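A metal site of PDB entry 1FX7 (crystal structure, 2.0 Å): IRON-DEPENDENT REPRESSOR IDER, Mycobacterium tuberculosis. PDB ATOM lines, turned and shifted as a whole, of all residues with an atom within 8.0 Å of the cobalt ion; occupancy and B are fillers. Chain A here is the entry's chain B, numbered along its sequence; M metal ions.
The side-chain carboxylate (OE1) of Glu 172 lies within salt-bridge range of the guanidinium group (NE) of Arg 80, 3.0 Å away. The backbone carbonyl oxygen (O) of Leu 170 sits at hydrogen-bond distance from the side-chain amide nitrogen (NE2) of Gln 175 (3.0 Å). A ring nitrogen (ND1) of His 79 sits at hydrogen-bond distance from the side-chain carboxylate of Glu 105, at 2.9 Å.
Within 4 Å of the cobalt ion: His 79, Glu 83, His 98, Glu 172 and Gln 175. Along chain A the residues within 4 Å of the cobalt ion span positions 79 to 175.
The cobalt ion is bound by ND1 of His 98 (1.9 Å), OE2 of Glu 83 (1.9 Å), OE2 of Glu 172 (2.1 Å), OE1 of Gln 175 (2.1 Å) and NE2 of His 79 (2.2 Å). The cobalt ion has five donor atoms within binding distance.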
ATOM      1  N   ARG A  13      19.911  12.728   8.271  1.00  0.00           N
ATOM      2  CA  ARG A  13      19.452  13.696   9.274  1.00  0.00           C
ATOM      3  C   ARG A  13      17.929  13.657   9.440  1.00  0.00           C
ATOM      4  O   ARG A  13      17.467  13.892  10.558  1.00  0.00           O
ATOM      5  CB  ARG A  13      19.947  15.126   9.014  1.00  0.00           C
ATOM      6  CG  ARG A  13      20.343  15.829  10.330  1.00  0.00           C
ATOM      7  CD  ARG A  13      20.148  17.346  10.187  1.00  0.00           C
ATOM      8  NE  ARG A  13      18.738  17.672  10.034  1.00  0.00           N
ATOM      9  CZ  ARG A  13      18.196  18.608   9.282  1.00  0.00           C
ATOM     10  NH1 ARG A  13      16.860  18.772   9.261  1.00  0.00           N
ATOM     11  NH2 ARG A  13      18.965  19.385   8.533  1.00  0.00           N
ATOM     12  N   ASP A  17      16.084  13.304  12.793  1.00  0.00           N
ATOM     13  CA  ASP A  17      15.084  14.306  13.163  1.00  0.00           C
ATOM     14  C   ASP A  17      13.807  13.595  13.645  1.00  0.00           C
ATOM     15  O   ASP A  17      13.254  13.907  14.698  1.00  0.00           O
ATOM     16  CB  ASP A  17      14.683  15.200  11.990  1.00  0.00           C
ATOM     17  CG  ASP A  17      15.679  16.257  11.540  1.00  0.00           C
ATOM     18  OD1 ASP A  17      16.654  16.584  12.238  1.00  0.00           O
ATOM     19  OD2 ASP A  17      15.488  16.817  10.441  1.00  0.00           O
ATOM     20  N   MET A  76      24.349  16.571  12.031  1.00  0.00           N
ATOM     21  CA  MET A  76      23.570  17.369  12.960  1.00  0.00           C
ATOM     22  C   MET A  76      24.458  18.280  13.787  1.00  0.00           C
ATOM     23  O   MET A  76      24.081  19.408  14.147  1.00  0.00           O
ATOM     24  CB  MET A  76      22.721  16.474  13.890  1.00  0.00           C
ATOM     25  CG  MET A  76      21.847  17.338  14.817  1.00  0.00           C
ATOM     26  SD  MET A  76      20.526  18.191  13.935  1.00  0.00           S
ATOM     27  CE  MET A  76      19.313  16.937  13.602  1.00  0.00           C
ATOM     28  N   HIS A  79      25.323  21.097  11.669  1.00  0.00           N
ATOM     29  CA  HIS A  79      24.134  21.924  11.586  1.00  0.00           C
ATOM     30  C   HIS A  79      23.960  22.868  12.765  1.00  0.00           C
ATOM     31  O   HIS A  79      23.705  24.054  12.553  1.00  0.00           O
ATOM     32  CB  HIS A  79      22.891  21.029  11.535  1.00  0.00           C
ATOM     33  CG  HIS A  79      21.617  21.793  11.333  1.00  0.00           C
ATOM     34  ND1 HIS A  79      21.100  22.060  10.081  1.00  0.00           N
ATOM     35  CD2 HIS A  79      20.759  22.359  12.209  1.00  0.00           C
ATOM     36  CE1 HIS A  79      19.971  22.731  10.205  1.00  0.00           C
ATOM     37  NE2 HIS A  79      19.746  22.910  11.489  1.00  0.00           N
ATOM     38  N   ARG A  80      24.049  22.345  13.987  1.00  0.00           N
ATOM     39  CA  ARG A  80      23.824  23.116  15.198  1.00  0.00           C
ATOM     40  C   ARG A  80      24.963  24.047  15.538  1.00  0.00           C
ATOM     41  O   ARG A  80      24.679  25.127  16.071  1.00  0.00           O
ATOM     42  CB  ARG A  80      23.432  22.153  16.356  1.00  0.00           C
ATOM     43  CG  ARG A  80      22.082  21.507  16.031  1.00  0.00           C
ATOM     44  CD  ARG A  80      21.556  20.532  17.095  1.00  0.00           C
ATOM     45  NE  ARG A  80      20.244  20.042  16.655  1.00  0.00           N
ATOM     46  CZ  ARG A  80      19.582  18.985  17.124  1.00  0.00           C
ATOM     47  NH1 ARG A  80      20.076  18.210  18.081  1.00  0.00           N
ATOM     48  NH2 ARG A  80      18.397  18.735  16.589  1.00  0.00           N
ATOM     49  N   GLU A  83      24.373  26.985  13.107  1.00  0.00           N
ATOM     50  CA  GLU A  83      23.302  27.844  13.607  1.00  0.00           C
ATOM     51  C   GLU A  83      23.815  28.757  14.726  1.00  0.00           C
ATOM     52  O   GLU A  83      23.462  29.947  14.740  1.00  0.00           O
ATOM     53  CB  GLU A  83      22.092  27.051  14.132  1.00  0.00           C
ATOM     54  CG  GLU A  83      21.255  26.390  13.065  1.00  0.00           C
ATOM     55  CD  GLU A  83      20.148  25.522  13.620  1.00  0.00           C
ATOM     56  OE1 GLU A  83      20.284  24.928  14.713  1.00  0.00           O
ATOM     57  OE2 GLU A  83      19.133  25.381  12.924  1.00  0.00           O
ATOM     58  N   TRP A  94      17.268  34.874  13.672  1.00  0.00           N
ATOM     59  CA  TRP A  94      16.967  33.602  14.274  1.00  0.00           C
ATOM     60  C   TRP A  94      16.164  32.691  13.371  1.00  0.00           C
ATOM     61  O   TRP A  94      16.553  31.549  13.152  1.00  0.00           O
ATOM     62  CB  TRP A  94      16.225  33.846  15.590  1.00  0.00           C
ATOM     63  CG  TRP A  94      16.240  32.757  16.617  1.00  0.00           C
ATOM     64  CD1 TRP A  94      17.314  32.263  17.306  1.00  0.00           C
ATOM     65  CD2 TRP A  94      15.093  32.067  17.135  1.00  0.00           C
ATOM     66  NE1 TRP A  94      16.911  31.289  18.203  1.00  0.00           N
ATOM     67  CE2 TRP A  94      15.547  31.150  18.098  1.00  0.00           C
ATOM     68  CE3 TRP A  94      13.726  32.131  16.856  1.00  0.00           C
ATOM     69  CZ2 TRP A  94      14.688  30.309  18.795  1.00  0.00           C
ATOM     70  CZ3 TRP A  94      12.875  31.302  17.551  1.00  0.00           C
ATOM     71  CH2 TRP A  94      13.349  30.397  18.514  1.00  0.00           C
ATOM     72  N   VAL A  97      18.276  31.140  10.338  1.00  0.00           N
ATOM     73  CA  VAL A  97      19.527  30.370  10.390  1.00  0.00           C
ATOM     74  C   VAL A  97      19.333  28.916  10.013  1.00  0.00           C
ATOM     75  O   VAL A  97      20.311  28.308   9.559  1.00  0.00           O
ATOM     76  CB  VAL A  97      20.280  30.509  11.714  1.00  0.00           C
ATOM     77  CG1 VAL A  97      20.509  32.001  12.012  1.00  0.00           C
ATOM     78  CG2 VAL A  97      19.526  29.849  12.890  1.00  0.00           C
ATOM     79  N   HIS A  98      18.135  28.361  10.197  1.00  0.00           N
ATOM     80  CA  HIS A  98      17.902  26.949   9.910  1.00  0.00           C
ATOM     81  C   HIS A  98      18.086  26.630   8.428  1.00  0.00           C
ATOM     82  O   HIS A  98      18.829  25.691   8.126  1.00  0.00           O
ATOM     83  CB  HIS A  98      16.506  26.462  10.386  1.00  0.00           C
ATOM     84  CG  HIS A  98      16.347  25.023   9.973  1.00  0.00           C
ATOM     85  ND1 HIS A  98      16.984  24.002  10.683  1.00  0.00           N
ATOM     86  CD2 HIS A  98      15.664  24.453   8.956  1.00  0.00           C
ATOM     87  CE1 HIS A  98      16.672  22.855  10.079  1.00  0.00           C
ATOM     88  NE2 HIS A  98      15.910  23.097   9.041  1.00  0.00           N
ATOM     89  N   ALA A  99      17.471  27.351   7.509  1.00  0.00           N
ATOM     90  CA  ALA A  99      17.617  27.065   6.077  1.00  0.00           C
ATOM     91  C   ALA A  99      19.077  27.192   5.688  1.00  0.00           C
ATOM     92  O   ALA A  99      19.616  26.368   4.944  1.00  0.00           O
ATOM     93  CB  ALA A  99      16.708  27.922   5.221  1.00  0.00           C
ATOM     94  N   GLU A 100      19.765  28.218   6.172  1.00  0.00           N
ATOM     95  CA  GLU A 100      21.187  28.409   5.866  1.00  0.00           C
ATOM     96  C   GLU A 100      21.997  27.230   6.394  1.00  0.00           C
ATOM     97  O   GLU A 100      22.729  26.561   5.674  1.00  0.00           O
ATOM     98  CB  GLU A 100      21.678  29.711   6.493  1.00  0.00           C
ATOM     99  CG  GLU A 100      23.036  30.132   5.951  1.00  0.00           C
ATOM    100  CD  GLU A 100      23.001  30.890   4.635  1.00  0.00           C
ATOM    101  OE1 GLU A 100      24.029  30.913   3.904  1.00  0.00           O
ATOM    102  OE2 GLU A 100      21.966  31.509   4.320  1.00  0.00           O
ATOM    103  N   ALA A 101      21.856  26.868   7.676  1.00  0.00           N
ATOM    104  CA  ALA A 101      22.563  25.759   8.285  1.00  0.00           C
ATOM    105  C   ALA A 101      22.253  24.422   7.617  1.00  0.00           C
ATOM    106  O   ALA A 101      23.114  23.537   7.535  1.00  0.00           O
ATOM    107  CB  ALA A 101      22.245  25.656   9.768  1.00  0.00           C
ATOM    108  N   CYS A 102      21.060  24.269   7.076  1.00  0.00           N
ATOM    109  CA  CYS A 102      20.697  23.047   6.362  1.00  0.00           C
ATOM    110  C   CYS A 102      21.581  22.917   5.124  1.00  0.00           C
ATOM    111  O   CYS A 102      21.893  21.795   4.725  1.00  0.00           O
ATOM    112  CB  CYS A 102      19.228  22.955   5.991  1.00  0.00           C
ATOM    113  SG  CYS A 102      18.732  21.232   5.524  1.00  0.00           S
ATOM    114  N   GLU A 105      25.647  22.489   6.676  1.00  0.00           N
ATOM    115  CA  GLU A 105      25.940  21.215   7.333  1.00  0.00           C
ATOM    116  C   GLU A 105      26.554  20.188   6.390  1.00  0.00           C
ATOM    117  O   GLU A 105      27.223  19.256   6.833  1.00  0.00           O
ATOM    118  CB  GLU A 105      24.660  20.664   7.973  1.00  0.00           C
ATOM    119  CG  GLU A 105      23.631  20.239   6.945  1.00  0.00           C
ATOM    120  CD  GLU A 105      22.281  19.821   7.482  1.00  0.00           C
ATOM    121  OE1 GLU A 105      22.188  19.723   8.710  1.00  0.00           O
ATOM    122  OE2 GLU A 105      21.330  19.593   6.677  1.00  0.00           O
ATOM    123  N   SER A 126      22.014  24.303  20.419  1.00  0.00           N
ATOM    124  CA  SER A 126      21.821  25.179  19.252  1.00  0.00           C
ATOM    125  C   SER A 126      20.994  26.378  19.710  1.00  0.00           C
ATOM    126  O   SER A 126      20.464  26.385  20.832  1.00  0.00           O
ATOM    127  CB  SER A 126      21.084  24.418  18.161  1.00  0.00           C
ATOM    128  OG  SER A 126      19.671  24.360  18.317  1.00  0.00           O
ATOM    129  N   PRO A 127      20.734  27.326  18.829  1.00  0.00           N
ATOM    130  CA  PRO A 127      19.911  28.485  19.146  1.00  0.00           C
ATOM    131  C   PRO A 127      18.472  28.103  19.453  1.00  0.00           C
ATOM    132  O   PRO A 127      17.745  28.911  20.001  1.00  0.00           O
ATOM    133  CB  PRO A 127      19.903  29.327  17.871  1.00  0.00           C
ATOM    134  CG  PRO A 127      21.173  28.919  17.164  1.00  0.00           C
ATOM    135  CD  PRO A 127      21.298  27.433  17.457  1.00  0.00           C
ATOM    136  N   PHE A 128      18.033  26.903  19.044  1.00  0.00           N
ATOM    137  CA  PHE A 128      16.698  26.429  19.300  1.00  0.00           C
ATOM    138  C   PHE A 128      16.671  25.502  20.502  1.00  0.00           C
ATOM    139  O   PHE A 128      15.685  24.805  20.720  1.00  0.00           O
ATOM    140  CB  PHE A 128      16.135  25.762  18.028  1.00  0.00           C
ATOM    141  CG  PHE A 128      15.992  26.770  16.922  1.00  0.00           C
ATOM    142  CD1 PHE A 128      17.015  26.951  15.993  1.00  0.00           C
ATOM    143  CD2 PHE A 128      14.861  27.561  16.836  1.00  0.00           C
ATOM    144  CE1 PHE A 128      16.879  27.889  14.978  1.00  0.00           C
ATOM    145  CE2 PHE A 128      14.717  28.506  15.830  1.00  0.00           C
ATOM    146  CZ  PHE A 128      15.739  28.663  14.908  1.00  0.00           C
ATOM    147  N   ASN A 130      18.282  22.743  21.127  1.00  0.00           N
ATOM    148  CA  ASN A 130      18.599  21.323  20.938  1.00  0.00           C
ATOM    149  C   ASN A 130      20.047  21.011  21.283  1.00  0.00           C
ATOM    150  O   ASN A 130      20.969  21.746  20.931  1.00  0.00           O
ATOM    151  CB  ASN A 130      18.339  20.876  19.512  1.00  0.00           C
ATOM    152  CG  ASN A 130      16.976  21.247  19.004  1.00  0.00           C
ATOM    153  OD1 ASN A 130      16.850  22.053  18.075  1.00  0.00           O
ATOM    154  ND2 ASN A 130      15.958  20.659  19.594  1.00  0.00           N
ATOM    155  N   LEU A 170      13.099  23.345  20.259  1.00  0.00           N
ATOM    156  CA  LEU A 170      12.269  23.413  19.060  1.00  0.00           C
ATOM    157  C   LEU A 170      13.099  22.602  18.052  1.00  0.00           C
ATOM    158  O   LEU A 170      14.159  23.115  17.642  1.00  0.00           O
ATOM    159  CB  LEU A 170      11.976  24.807  18.549  1.00  0.00           C
ATOM    160  CG  LEU A 170      11.120  25.723  19.452  1.00  0.00           C
ATOM    161  CD1 LEU A 170      12.041  26.494  20.396  1.00  0.00           C
ATOM    162  CD2 LEU A 170      10.288  26.690  18.630  1.00  0.00           C
ATOM    163  N   THR A 171      12.711  21.379  17.764  1.00  0.00           N
ATOM    164  CA  THR A 171      13.552  20.523  16.902  1.00  0.00           C
ATOM    165  C   THR A 171      13.553  20.965  15.464  1.00  0.00           C
ATOM    166  O   THR A 171      12.804  21.873  15.075  1.00  0.00           O
ATOM    167  CB  THR A 171      13.184  19.029  17.063  1.00  0.00           C
ATOM    168  OG1 THR A 171      11.919  18.788  16.450  1.00  0.00           O
ATOM    169  CG2 THR A 171      13.136  18.684  18.549  1.00  0.00           C
ATOM    170  N   GLU A 172      14.347  20.306  14.600  1.00  0.00           N
ATOM    171  CA  GLU A 172      14.474  20.750  13.221  1.00  0.00           C
ATOM    172  C   GLU A 172      13.211  20.778  12.397  1.00  0.00           C
ATOM    173  O   GLU A 172      13.105  21.655  11.510  1.00  0.00           O
ATOM    174  CB  GLU A 172      15.576  19.977  12.492  1.00  0.00           C
ATOM    175  CG  GLU A 172      16.869  19.805  13.281  1.00  0.00           C
ATOM    176  CD  GLU A 172      17.516  21.119  13.681  1.00  0.00           C
ATOM    177  OE1 GLU A 172      18.298  21.154  14.650  1.00  0.00           O
ATOM    178  OE2 GLU A 172      17.212  22.116  12.997  1.00  0.00           O
ATOM    179  N   HIS A 173      12.235  19.909  12.626  1.00  0.00           N
ATOM    180  CA  HIS A 173      11.032  19.923  11.792  1.00  0.00           C
ATOM    181  C   HIS A 173      10.303  21.258  11.882  1.00  0.00           C
ATOM    182  O   HIS A 173       9.858  21.777  10.848  1.00  0.00           O
ATOM    183  CB  HIS A 173      10.073  18.778  12.166  1.00  0.00           C
ATOM    184  CG  HIS A 173       8.941  18.620  11.196  1.00  0.00           C
ATOM    185  ND1 HIS A 173       9.145  18.618   9.847  1.00  0.00           N
ATOM    186  CD2 HIS A 173       7.608  18.416  11.369  1.00  0.00           C
ATOM    187  CE1 HIS A 173       7.997  18.469   9.209  1.00  0.00           C
ATOM    188  NE2 HIS A 173       7.056  18.343  10.117  1.00  0.00           N
ATOM    189  N   VAL A 174      10.111  21.767  13.101  1.00  0.00           N
ATOM    190  CA  VAL A 174       9.354  23.020  13.242  1.00  0.00           C
ATOM    191  C   VAL A 174      10.132  24.213  12.710  1.00  0.00           C
ATOM    192  O   VAL A 174       9.496  25.164  12.248  1.00  0.00           O
ATOM    193  CB  VAL A 174       8.822  23.223  14.671  1.00  0.00           C
ATOM    194  CG1 VAL A 174       9.915  23.391  15.698  1.00  0.00           C
ATOM    195  CG2 VAL A 174       7.849  24.386  14.744  1.00  0.00           C
ATOM    196  N   GLN A 175      11.456  24.154  12.665  1.00  0.00           N
ATOM    197  CA  GLN A 175      12.239  25.258  12.081  1.00  0.00           C
ATOM    198  C   GLN A 175      12.036  25.335  10.584  1.00  0.00           C
ATOM    199  O   GLN A 175      12.214  26.409  10.008  1.00  0.00           O
ATOM    200  CB  GLN A 175      13.739  25.102  12.352  1.00  0.00           C
ATOM    201  CG  GLN A 175      14.099  24.997  13.813  1.00  0.00           C
ATOM    202  CD  GLN A 175      15.520  24.584  14.075  1.00  0.00           C
ATOM    203  OE1 GLN A 175      16.404  24.883  13.268  1.00  0.00           O
ATOM    204  NE2 GLN A 175      15.734  23.895  15.187  1.00  0.00           N
ATOM    205  N   GLY A 176      11.638  24.239   9.930  1.00  0.00           N
ATOM    206  CA  GLY A 176      11.397  24.194   8.506  1.00  0.00           C
ATOM    207  C   GLY A 176      10.165  24.976   8.060  1.00  0.00           C
ATOM    208  O   GLY A 176       9.988  25.258   6.878  1.00  0.00           O
HETATM  209 CO    CO M   1      18.000  23.910  12.336  1.00  0.00          CO
